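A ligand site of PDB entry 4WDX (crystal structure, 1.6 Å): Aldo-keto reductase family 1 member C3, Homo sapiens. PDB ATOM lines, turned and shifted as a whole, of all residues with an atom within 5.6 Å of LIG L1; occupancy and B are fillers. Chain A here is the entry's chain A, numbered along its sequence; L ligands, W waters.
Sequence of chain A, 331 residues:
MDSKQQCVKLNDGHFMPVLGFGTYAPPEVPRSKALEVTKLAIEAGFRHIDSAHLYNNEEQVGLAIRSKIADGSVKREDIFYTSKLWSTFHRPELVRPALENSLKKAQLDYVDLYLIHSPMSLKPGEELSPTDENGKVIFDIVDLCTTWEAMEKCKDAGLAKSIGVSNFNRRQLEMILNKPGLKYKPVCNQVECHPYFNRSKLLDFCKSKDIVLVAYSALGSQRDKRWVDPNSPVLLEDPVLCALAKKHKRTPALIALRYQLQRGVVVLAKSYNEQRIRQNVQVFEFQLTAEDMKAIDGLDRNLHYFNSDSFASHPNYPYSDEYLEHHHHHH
The side-chain hydroxyl of Ser 118 lies close to the backbone NH of Met 120, 3.2 Å away. The side-chain amide nitrogen (ND2) of Asn 167 lies within hydrogen-bond range of the backbone carbonyl oxygen (O) of His 117 (3.1 Å). The side-chain hydroxyl (OG) of Ser 221 is in hydrogen-bond range of the backbone NH (N) of Arg 223, 3.0 Å away. The side-chain hydroxyl (OH) of Tyr 216 is in hydrogen-bond range of the side-chain amide oxygen (OD1) of Asn 167, 2.5 Å away. The backbone carbonyl oxygen (O) of Tyr 24 sits at hydrogen-bond distance from the side-chain amide nitrogen (NE2) of Gln 222 (2.7 Å). NZ of Lys 84 is in hydrogen-bond range of OH of Tyr 55. O of Met 120 lies within hydrogen-bond range of OG of Ser 87.
Water W1 lies within hydrogen-bond range of an oxygen (O2) of LIG L1 (2.9 Å), the backbone NH (N) of Asp 224 (3.1 Å) and the backbone NH (N) of Arg 223 (3.2 Å).
O2 of LIG L1 sits at hydrogen-bond distance from O8 of LG2 L2 (2.7 Å).
Tyr 24 touches LIG L1 (CD2 to C11, 3.5 Å). CD2 of Leu 54 touches C4 of LIG L1, 3.4 Å away. Trp 86 touches LIG L1 (CH2 to C3, 3.6 Å). Ser 118 touches LIG L1 (CB to C1, 3.5 Å). Met 120 touches LIG L1. Asn 167 touches LIG L1 (ND2 to C2, 3.6 Å). Ser 221 touches LIG L1. CZ3 of Trp 227 touches C14 of LIG L1, at 3.5 Å. Phe 306 touches LIG L1. Ser 308 touches LIG L1 (CB to C1, 3.8 Å). Phe 311 touches LIG L1. Of the 20 residues printed, 14 come within 4 Å of LIG L1. The nearest printed residue that does not touch LIG L1 is Ser 217 (4.3 Å).
An oxygen (O8) of LG2 L2 sits at hydrogen-bond distance from the side-chain hydroxyl (OG) of Ser 217, at 2.9 Å. N of Ser 217 lies within hydrogen-bond range of O10 of LG2 L2 (3.1 Å). A ring nitrogen (NE2) of His 117 is in hydrogen-bond range of an oxygen (O1) of LIG L1 (2.8 Å). The backbone NH of Tyr 24 sits at hydrogen-bond distance from an oxygen (O12) of LG2 L2, at 3.1 Å. The backbone NH (N) of Gln 222 sits at hydrogen-bond distance from an oxygen (O2) of LIG L1, 3.1 Å away. N of Ser 221 is in hydrogen-bond range of O1 of LG2 L2. The side-chain amide nitrogen (NE2) of Gln 222 is in hydrogen-bond range of an oxygen (O9) of LG2 L2 (2.8 Å). The side-chain amide nitrogen (ND2) of Asn 167 sits at hydrogen-bond distance from an oxygen (O14) of LG2 L2, 2.7 Å away. The side-chain hydroxyl (OH) of Tyr 55 is in hydrogen-bond range of an oxygen (O1) of LIG L1. A ring nitrogen (NE2) of His 117 is in hydrogen-bond range of an oxygen (O14) of LG2 L2, 3.4 Å away.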
ATOM      1  N   TYR A  24       7.954  12.183  11.630  1.00  0.00           N
ATOM      2  CA  TYR A  24       9.347  12.344  12.043  1.00  0.00           C
ATOM      3  C   TYR A  24       9.450  12.328  13.532  1.00  0.00           C
ATOM      4  O   TYR A  24       8.777  13.103  14.232  1.00  0.00           O
ATOM      5  CB  TYR A  24       9.977  13.595  11.485  1.00  0.00           C
ATOM      6  CG  TYR A  24      11.388  13.697  11.980  1.00  0.00           C
ATOM      7  CD1 TYR A  24      12.383  12.870  11.415  1.00  0.00           C
ATOM      8  CD2 TYR A  24      11.696  14.539  13.040  1.00  0.00           C
ATOM      9  CE1 TYR A  24      13.716  12.919  11.918  1.00  0.00           C
ATOM     10  CE2 TYR A  24      13.050  14.583  13.549  1.00  0.00           C
ATOM     11  CZ  TYR A  24      14.016  13.765  12.944  1.00  0.00           C
ATOM     12  OH  TYR A  24      15.394  13.804  13.381  1.00  0.00           O
ATOM     13  N   LEU A  54      14.687   9.894   4.687  1.00  0.00           N
ATOM     14  CA  LEU A  54      15.518  10.464   5.738  1.00  0.00           C
ATOM     15  C   LEU A  54      15.069  10.093   7.115  1.00  0.00           C
ATOM     16  O   LEU A  54      15.869  10.075   8.075  1.00  0.00           O
ATOM     17  CB  LEU A  54      15.489  11.990   5.556  1.00  0.00           C
ATOM     18  CG  LEU A  54      16.365  12.788   6.522  1.00  0.00           C
ATOM     19  CD1 LEU A  54      17.782  12.608   5.993  1.00  0.00           C
ATOM     20  CD2 LEU A  54      15.949  14.251   6.493  1.00  0.00           C
ATOM     21  N   TYR A  55      13.766   9.802   7.253  1.00  0.00           N
ATOM     22  CA  TYR A  55      13.279   9.637   8.597  1.00  0.00           C
ATOM     23  C   TYR A  55      13.629   8.297   9.221  1.00  0.00           C
ATOM     24  O   TYR A  55      13.306   8.097  10.366  1.00  0.00           O
ATOM     25  CB  TYR A  55      11.750   9.887   8.715  1.00  0.00           C
ATOM     26  CG  TYR A  55      11.287  11.232   8.153  1.00  0.00           C
ATOM     27  CD1 TYR A  55       9.918  11.463   7.902  1.00  0.00           C
ATOM     28  CD2 TYR A  55      12.171  12.268   7.902  1.00  0.00           C
ATOM     29  CE1 TYR A  55       9.477  12.710   7.378  1.00  0.00           C
ATOM     30  CE2 TYR A  55      11.736  13.463   7.326  1.00  0.00           C
ATOM     31  CZ  TYR A  55      10.409  13.683   7.088  1.00  0.00           C
ATOM     32  OH  TYR A  55      10.029  14.903   6.596  1.00  0.00           O
ATOM     33  N   LYS A  84       9.622  10.688   0.286  1.00  0.00           N
ATOM     34  CA  LYS A  84      10.349  11.783  -0.331  1.00  0.00           C
ATOM     35  C   LYS A  84      11.731  11.227  -0.737  1.00  0.00           C
ATOM     36  O   LYS A  84      12.349  10.446   0.031  1.00  0.00           O
ATOM     37  CB  LYS A  84      10.545  12.921   0.696  1.00  0.00           C
ATOM     38  CG  LYS A  84       9.192  13.390   1.388  1.00  0.00           C
ATOM     39  CD  LYS A  84       9.371  14.672   2.222  1.00  0.00           C
ATOM     40  CE  LYS A  84       8.144  15.002   3.082  1.00  0.00           C
ATOM     41  NZ  LYS A  84       8.063  14.213   4.380  1.00  0.00           N
ATOM     42  N   TRP A  86      15.463  11.670  -1.175  1.00  0.00           N
ATOM     43  CA  TRP A  86      16.480  12.346  -0.439  1.00  0.00           C
ATOM     44  C   TRP A  86      17.577  12.988  -1.370  1.00  0.00           C
ATOM     45  O   TRP A  86      17.634  12.677  -2.545  1.00  0.00           O
ATOM     46  CB  TRP A  86      17.117  11.407   0.635  1.00  0.00           C
ATOM     47  CG  TRP A  86      18.170  12.156   1.444  1.00  0.00           C
ATOM     48  CD1 TRP A  86      19.520  11.821   1.521  1.00  0.00           C
ATOM     49  CD2 TRP A  86      18.036  13.405   2.168  1.00  0.00           C
ATOM     50  NE1 TRP A  86      20.181  12.739   2.274  1.00  0.00           N
ATOM     51  CE2 TRP A  86      19.343  13.728   2.690  1.00  0.00           C
ATOM     52  CE3 TRP A  86      16.971  14.298   2.441  1.00  0.00           C
ATOM     53  CZ2 TRP A  86      19.596  14.880   3.467  1.00  0.00           C
ATOM     54  CZ3 TRP A  86      17.224  15.419   3.224  1.00  0.00           C
ATOM     55  CH2 TRP A  86      18.539  15.721   3.716  1.00  0.00           C
ATOM     56  N   SER A  87      18.333  13.920  -0.833  1.00  0.00           N
ATOM     57  CA  SER A  87      19.207  14.851  -1.668  1.00  0.00           C
ATOM     58  C   SER A  87      20.463  14.123  -2.154  1.00  0.00           C
ATOM     59  O   SER A  87      21.055  14.480  -3.197  1.00  0.00           O
ATOM     60  CB  SER A  87      19.573  16.099  -0.863  1.00  0.00           C
ATOM     61  OG  SER A  87      18.419  16.999  -0.792  1.00  0.00           O
ATOM     62  N   HIS A 117      12.618  16.004  -1.797  1.00  0.00           N
ATOM     63  CA  HIS A 117      12.654  16.451  -0.429  1.00  0.00           C
ATOM     64  C   HIS A 117      13.195  17.922  -0.310  1.00  0.00           C
ATOM     65  O   HIS A 117      12.712  18.709   0.503  1.00  0.00           O
ATOM     66  CB  HIS A 117      13.472  15.453   0.451  1.00  0.00           C
ATOM     67  CG  HIS A 117      13.199  15.510   1.930  1.00  0.00           C
ATOM     68  ND1 HIS A 117      13.289  14.383   2.741  1.00  0.00           N
ATOM     69  CD2 HIS A 117      12.870  16.536   2.753  1.00  0.00           C
ATOM     70  CE1 HIS A 117      13.067  14.722   3.994  1.00  0.00           C
ATOM     71  NE2 HIS A 117      12.807  16.032   4.025  1.00  0.00           N
ATOM     72  N   SER A 118      14.216  18.260  -1.129  1.00  0.00           N
ATOM     73  CA  SER A 118      14.767  19.595  -1.016  1.00  0.00           C
ATOM     74  C   SER A 118      15.425  19.873  -2.390  1.00  0.00           C
ATOM     75  O   SER A 118      15.834  18.936  -3.078  1.00  0.00           O
ATOM     76  CB  SER A 118      15.756  19.596   0.179  1.00  0.00           C
ATOM     77  OG  SER A 118      16.873  20.438  -0.003  1.00  0.00           O
ATOM     78  N   MET A 120      18.284  21.147  -2.778  1.00  0.00           N
ATOM     79  CA  MET A 120      19.734  20.879  -2.638  1.00  0.00           C
ATOM     80  C   MET A 120      20.101  19.473  -3.151  1.00  0.00           C
ATOM     81  O   MET A 120      19.337  18.531  -2.880  1.00  0.00           O
ATOM     82  CB  MET A 120      20.068  21.064  -1.171  1.00  0.00           C
ATOM     83  CG  MET A 120      21.531  20.869  -0.802  1.00  0.00           C
ATOM     84  SD  MET A 120      21.577  20.828   0.993  1.00  0.00           S
ATOM     85  CE  MET A 120      21.024  22.497   1.452  1.00  0.00           C
ATOM     86  N   ASN A 167      10.111  22.208  -0.038  1.00  0.00           N
ATOM     87  CA  ASN A 167      11.114  23.241   0.252  1.00  0.00           C
ATOM     88  C   ASN A 167      11.538  24.046  -0.973  1.00  0.00           C
ATOM     89  O   ASN A 167      12.652  24.567  -1.053  1.00  0.00           O
ATOM     90  CB  ASN A 167      12.345  22.618   0.982  1.00  0.00           C
ATOM     91  CG  ASN A 167      12.023  22.214   2.424  1.00  0.00           C
ATOM     92  OD1 ASN A 167      11.727  23.046   3.273  1.00  0.00           O
ATOM     93  ND2 ASN A 167      12.078  20.875   2.676  1.00  0.00           N
ATOM     94  N   TYR A 216       4.322  22.044   6.742  1.00  0.00           N
ATOM     95  CA  TYR A 216       4.999  21.270   7.806  1.00  0.00           C
ATOM     96  C   TYR A 216       5.500  22.220   8.856  1.00  0.00           C
ATOM     97  O   TYR A 216       5.599  23.419   8.578  1.00  0.00           O
ATOM     98  CB  TYR A 216       6.193  20.520   7.187  1.00  0.00           C
ATOM     99  CG  TYR A 216       7.443  21.274   6.763  1.00  0.00           C
ATOM    100  CD1 TYR A 216       7.835  21.318   5.426  1.00  0.00           C
ATOM    101  CD2 TYR A 216       8.296  21.862   7.723  1.00  0.00           C
ATOM    102  CE1 TYR A 216       9.069  21.880   5.038  1.00  0.00           C
ATOM    103  CE2 TYR A 216       9.521  22.446   7.336  1.00  0.00           C
ATOM    104  CZ  TYR A 216       9.881  22.477   6.014  1.00  0.00           C
ATOM    105  OH  TYR A 216      11.079  23.088   5.665  1.00  0.00           O
ATOM    106  N   SER A 217       5.794  21.702  10.043  1.00  0.00           N
ATOM    107  CA  SER A 217       5.950  22.453  11.283  1.00  0.00           C
ATOM    108  C   SER A 217       4.844  23.430  11.504  1.00  0.00           C
ATOM    109  O   SER A 217       5.064  24.526  12.018  1.00  0.00           O
ATOM    110  CB  SER A 217       7.360  23.134  11.368  1.00  0.00           C
ATOM    111  OG  SER A 217       8.383  22.084  11.169  1.00  0.00           O
ATOM    112  N   SER A 221       6.945  23.326  15.144  1.00  0.00           N
ATOM    113  CA  SER A 221       8.127  22.387  15.120  1.00  0.00           C
ATOM    114  C   SER A 221       8.279  21.673  16.462  1.00  0.00           C
ATOM    115  O   SER A 221       7.640  21.987  17.510  1.00  0.00           O
ATOM    116  CB  SER A 221       9.425  23.069  14.671  1.00  0.00           C
ATOM    117  OG  SER A 221      10.055  23.664  15.823  1.00  0.00           O
ATOM    118  N   GLN A 222       9.056  20.608  16.385  1.00  0.00           N
ATOM    119  CA  GLN A 222       9.418  19.838  17.532  1.00  0.00           C
ATOM    120  C   GLN A 222      10.510  20.597  18.361  1.00  0.00           C
ATOM    121  O   GLN A 222      10.777  20.160  19.482  1.00  0.00           O
ATOM    122  CB  GLN A 222       9.964  18.469  17.077  1.00  0.00           C
ATOM    123  CG  GLN A 222       8.927  17.666  16.252  1.00  0.00           C
ATOM    124  CD  GLN A 222       9.278  16.226  16.043  1.00  0.00           C
ATOM    125  OE1 GLN A 222       9.851  15.534  16.944  1.00  0.00           O
ATOM    126  NE2 GLN A 222       8.938  15.694  14.839  1.00  0.00           N
ATOM    127  N   ARG A 223      10.965  21.744  17.884  1.00  0.00           N
ATOM    128  CA  ARG A 223      11.959  22.611  18.671  1.00  0.00           C
ATOM    129  C   ARG A 223      13.191  21.741  19.044  1.00  0.00           C
ATOM    130  O   ARG A 223      13.733  21.772  20.158  1.00  0.00           O
ATOM    131  CB  ARG A 223      11.286  23.227  19.902  1.00  0.00           C
ATOM    132  CG  ARG A 223      10.085  24.129  19.578  1.00  0.00           C
ATOM    133  CD  ARG A 223       9.499  24.701  20.854  1.00  0.00           C
ATOM    134  NE  ARG A 223      10.490  25.606  21.417  1.00  0.00           N
ATOM    135  CZ  ARG A 223      10.734  26.855  21.029  1.00  0.00           C
ATOM    136  NH1 ARG A 223      11.719  27.543  21.640  1.00  0.00           N
ATOM    137  NH2 ARG A 223      10.023  27.418  20.030  1.00  0.00           N
ATOM    138  N   ASP A 224      13.621  20.940  18.092  1.00  0.00           N
ATOM    139  CA  ASP A 224      14.763  20.055  18.319  1.00  0.00           C
ATOM    140  C   ASP A 224      16.020  20.936  18.460  1.00  0.00           C
ATOM    141  O   ASP A 224      16.281  21.833  17.627  1.00  0.00           O
ATOM    142  CB  ASP A 224      14.893  19.118  17.139  1.00  0.00           C
ATOM    143  CG  ASP A 224      15.864  17.944  17.419  1.00  0.00           C
ATOM    144  OD1 ASP A 224      15.460  16.734  17.453  1.00  0.00           O
ATOM    145  OD2 ASP A 224      17.070  18.231  17.532  1.00  0.00           O
ATOM    146  N   TRP A 227      18.304  22.366  15.742  1.00  0.00           N
ATOM    147  CA  TRP A 227      17.942  23.350  14.702  1.00  0.00           C
ATOM    148  C   TRP A 227      17.182  24.541  15.271  1.00  0.00           C
ATOM    149  O   TRP A 227      16.850  25.498  14.548  1.00  0.00           O
ATOM    150  CB  TRP A 227      17.034  22.675  13.657  1.00  0.00           C
ATOM    151  CG  TRP A 227      17.535  21.353  13.071  1.00  0.00           C
ATOM    152  CD1 TRP A 227      18.648  21.161  12.327  1.00  0.00           C
ATOM    153  CD2 TRP A 227      16.873  20.091  13.155  1.00  0.00           C
ATOM    154  NE1 TRP A 227      18.743  19.840  11.934  1.00  0.00           N
ATOM    155  CE2 TRP A 227      17.666  19.154  12.431  1.00  0.00           C
ATOM    156  CE3 TRP A 227      15.680  19.658  13.759  1.00  0.00           C
ATOM    157  CZ2 TRP A 227      17.318  17.791  12.302  1.00  0.00           C
ATOM    158  CZ3 TRP A 227      15.355  18.288  13.663  1.00  0.00           C
ATOM    159  CH2 TRP A 227      16.163  17.388  12.919  1.00  0.00           C
ATOM    160  N   PHE A 306      13.066  25.786  11.036  1.00  0.00           N
ATOM    161  CA  PHE A 306      14.102  24.962  10.385  1.00  0.00           C
ATOM    162  C   PHE A 306      14.794  25.789   9.341  1.00  0.00           C
ATOM    163  O   PHE A 306      14.155  26.534   8.614  1.00  0.00           O
ATOM    164  CB  PHE A 306      13.470  23.704   9.725  1.00  0.00           C
ATOM    165  CG  PHE A 306      14.494  22.769   9.098  1.00  0.00           C
ATOM    166  CD1 PHE A 306      15.419  22.107   9.888  1.00  0.00           C
ATOM    167  CD2 PHE A 306      14.517  22.565   7.709  1.00  0.00           C
ATOM    168  CE1 PHE A 306      16.335  21.228   9.317  1.00  0.00           C
ATOM    169  CE2 PHE A 306      15.478  21.727   7.116  1.00  0.00           C
ATOM    170  CZ  PHE A 306      16.383  21.038   7.934  1.00  0.00           C
ATOM    171  N   SER A 308      17.452  25.004   6.285  1.00  0.00           N
ATOM    172  CA  SER A 308      18.181  23.946   5.623  1.00  0.00           C
ATOM    173  C   SER A 308      19.692  24.254   5.612  1.00  0.00           C
ATOM    174  O   SER A 308      20.495  23.303   5.645  1.00  0.00           O
ATOM    175  CB  SER A 308      17.652  23.725   4.205  1.00  0.00           C
ATOM    176  OG  SER A 308      17.087  24.927   3.754  1.00  0.00           O
ATOM    177  N   PHE A 311      21.299  22.313   8.190  1.00  0.00           N
ATOM    178  CA  PHE A 311      21.263  20.864   8.003  1.00  0.00           C
ATOM    179  C   PHE A 311      21.379  20.559   6.485  1.00  0.00           C
ATOM    180  O   PHE A 311      21.717  19.436   6.055  1.00  0.00           O
ATOM    181  CB  PHE A 311      19.959  20.272   8.604  1.00  0.00           C
ATOM    182  CG  PHE A 311      19.767  18.803   8.309  1.00  0.00           C
ATOM    183  CD1 PHE A 311      18.913  18.023   9.077  1.00  0.00           C
ATOM    184  CD2 PHE A 311      20.499  18.177   7.294  1.00  0.00           C
ATOM    185  CE1 PHE A 311      18.798  16.678   8.840  1.00  0.00           C
ATOM    186  CE2 PHE A 311      20.385  16.842   7.029  1.00  0.00           C
ATOM    187  CZ  PHE A 311      19.529  16.084   7.805  1.00  0.00           C
HETATM  188  C1  LIG L   1      16.546  20.122   3.503  1.00  0.00           C
HETATM  189  C2  LIG L   1      15.238  19.795   3.888  1.00  0.00           C
HETATM  190  C3  LIG L   1      17.555  18.784   5.256  1.00  0.00           C
HETATM  191  C4  LIG L   1      15.809  17.648   6.732  1.00  0.00           C
HETATM  192  C5  LIG L   1      16.250  18.465   5.669  1.00  0.00           C
HETATM  193  C6  LIG L   1      17.651  19.625   4.165  1.00  0.00           C
HETATM  194  C7  LIG L   1      15.151  18.961   4.986  1.00  0.00           C
HETATM  195  C8  LIG L   1      14.404  17.666   6.680  1.00  0.00           C
HETATM  196  C9  LIG L   1      13.417  16.991   7.472  1.00  0.00           C
HETATM  197  C10 LIG L   1      13.720  18.649  10.362  1.00  0.00           C
HETATM  198  C11 LIG L   1      11.841  17.015  10.543  1.00  0.00           C
HETATM  199  C12 LIG L   1      14.574  17.646   9.597  1.00  0.00           C
HETATM  200  C13 LIG L   1      12.606  16.133   9.567  1.00  0.00           C
HETATM  201  C14 LIG L   1      12.773  17.927  11.348  1.00  0.00           C
HETATM  202  C15 LIG L   1      19.034  20.009   3.687  1.00  0.00           C
HETATM  203  C16 LIG L   1      11.956  18.974  12.056  1.00  0.00           C
HETATM  204  C17 LIG L   1      11.169  18.394  13.212  1.00  0.00           C
HETATM  205  N1  LIG L   1      14.033  18.467   5.627  1.00  0.00           N
HETATM  206  N2  LIG L   1      13.634  16.817   8.809  1.00  0.00           N
HETATM  207  O1  LIG L   1      12.469  16.553   6.805  1.00  0.00           O
HETATM  208  O2  LIG L   1      10.434  19.421  13.915  1.00  0.00           O
HETATM  209  P1  LG2 L   2       4.646  19.827  14.266  1.00  0.00           P
HETATM  210  O1  LG2 L   2       4.956  21.244  13.932  1.00  0.00           O
HETATM  211  O2  LG2 L   2       3.518  19.179  13.492  1.00  0.00           O
HETATM  212  O3  LG2 L   2       4.337  19.439  15.743  1.00  0.00           O
HETATM  213  C1  LG2 L   2       5.235  20.056  16.723  1.00  0.00           C
HETATM  214  C2  LG2 L   2       4.944  19.442  18.057  1.00  0.00           C
HETATM  215  O4  LG2 L   2       3.578  19.685  18.430  1.00  0.00           O
HETATM  216  C3  LG2 L   2       5.058  17.959  18.146  1.00  0.00           C
HETATM  217  O5  LG2 L   2       6.392  17.526  18.553  1.00  0.00           O
HETATM  218  C4  LG2 L   2       3.970  17.500  19.091  1.00  0.00           C
HETATM  219  O6  LG2 L   2       4.501  16.902  20.302  1.00  0.00           O
HETATM  220  C5  LG2 L   2       3.212  18.780  19.387  1.00  0.00           C
HETATM  221  N1  LG2 L   2       1.787  18.640  19.267  1.00  0.00           N
HETATM  222  C6  LG2 L   2       1.108  17.897  18.302  1.00  0.00           C
HETATM  223  N2  LG2 L   2      -0.178  18.022  18.512  1.00  0.00           N
HETATM  224  C7  LG2 L   2      -0.383  18.846  19.620  1.00  0.00           C
HETATM  225  C8  LG2 L   2      -1.516  19.291  20.310  1.00  0.00           C
HETATM  226  N3  LG2 L   2      -2.905  19.003  20.020  1.00  0.00           N
HETATM  227  N4  LG2 L   2      -1.309  20.075  21.400  1.00  0.00           N
HETATM  228  C9  LG2 L   2      -0.048  20.393  21.746  1.00  0.00           C
HETATM  229  N5  LG2 L   2       1.096  20.005  21.150  1.00  0.00           N
HETATM  230  C10 LG2 L   2       0.855  19.228  20.082  1.00  0.00           C
HETATM  231  O7  LG2 L   2       5.971  18.902  13.947  1.00  0.00           O
HETATM  232  P2  LG2 L   2       7.046  18.720  12.801  1.00  0.00           P
HETATM  233  O8  LG2 L   2       8.003  19.842  12.898  1.00  0.00           O
HETATM  234  O9  LG2 L   2       7.469  17.312  13.016  1.00  0.00           O
HETATM  235  O10 LG2 L   2       6.204  18.915  11.417  1.00  0.00           O
HETATM  236  C11 LG2 L   2       5.322  17.800  11.169  1.00  0.00           C
HETATM  237  C12 LG2 L   2       5.792  16.870  10.061  1.00  0.00           C
HETATM  238  O11 LG2 L   2       6.049  17.531   8.837  1.00  0.00           O
HETATM  239  C13 LG2 L   2       7.093  16.070  10.279  1.00  0.00           C
HETATM  240  O12 LG2 L   2       6.891  15.070  11.347  1.00  0.00           O
HETATM  241  C14 LG2 L   2       7.398  15.591   8.882  1.00  0.00           C
HETATM  242  O13 LG2 L   2       6.493  14.482   8.599  1.00  0.00           O
HETATM  243  C15 LG2 L   2       7.034  16.857   8.044  1.00  0.00           C
HETATM  244  N6  LG2 L   2       8.194  17.762   7.850  1.00  0.00           N
HETATM  245  C16 LG2 L   2       8.782  17.836   6.640  1.00  0.00           C
HETATM  246  C17 LG2 L   2       9.899  18.640   6.372  1.00  0.00           C
HETATM  247  C18 LG2 L   2      10.439  18.700   5.016  1.00  0.00           C
HETATM  248  O14 LG2 L   2      11.544  19.137   4.699  1.00  0.00           O
HETATM  249  N7  LG2 L   2       9.495  18.361   4.062  1.00  0.00           N
HETATM  250  C19 LG2 L   2      10.503  19.359   7.410  1.00  0.00           C
HETATM  251  C20 LG2 L   2       9.835  19.283   8.629  1.00  0.00           C
HETATM  252  C21 LG2 L   2       8.701  18.505   8.863  1.00  0.00           C
HETATM  253  P3  LG2 L   2       3.946  15.439  20.778  1.00  0.00           P
HETATM  254  O15 LG2 L   2       4.563  14.429  19.789  1.00  0.00           O
HETATM  255  O16 LG2 L   2       4.570  15.359  22.203  1.00  0.00           O
HETATM  256  O17 LG2 L   2       2.425  15.481  20.902  1.00  0.00           O
HETATM  257  O   HOH W   1      12.529  20.877  15.235  1.00  0.00           O
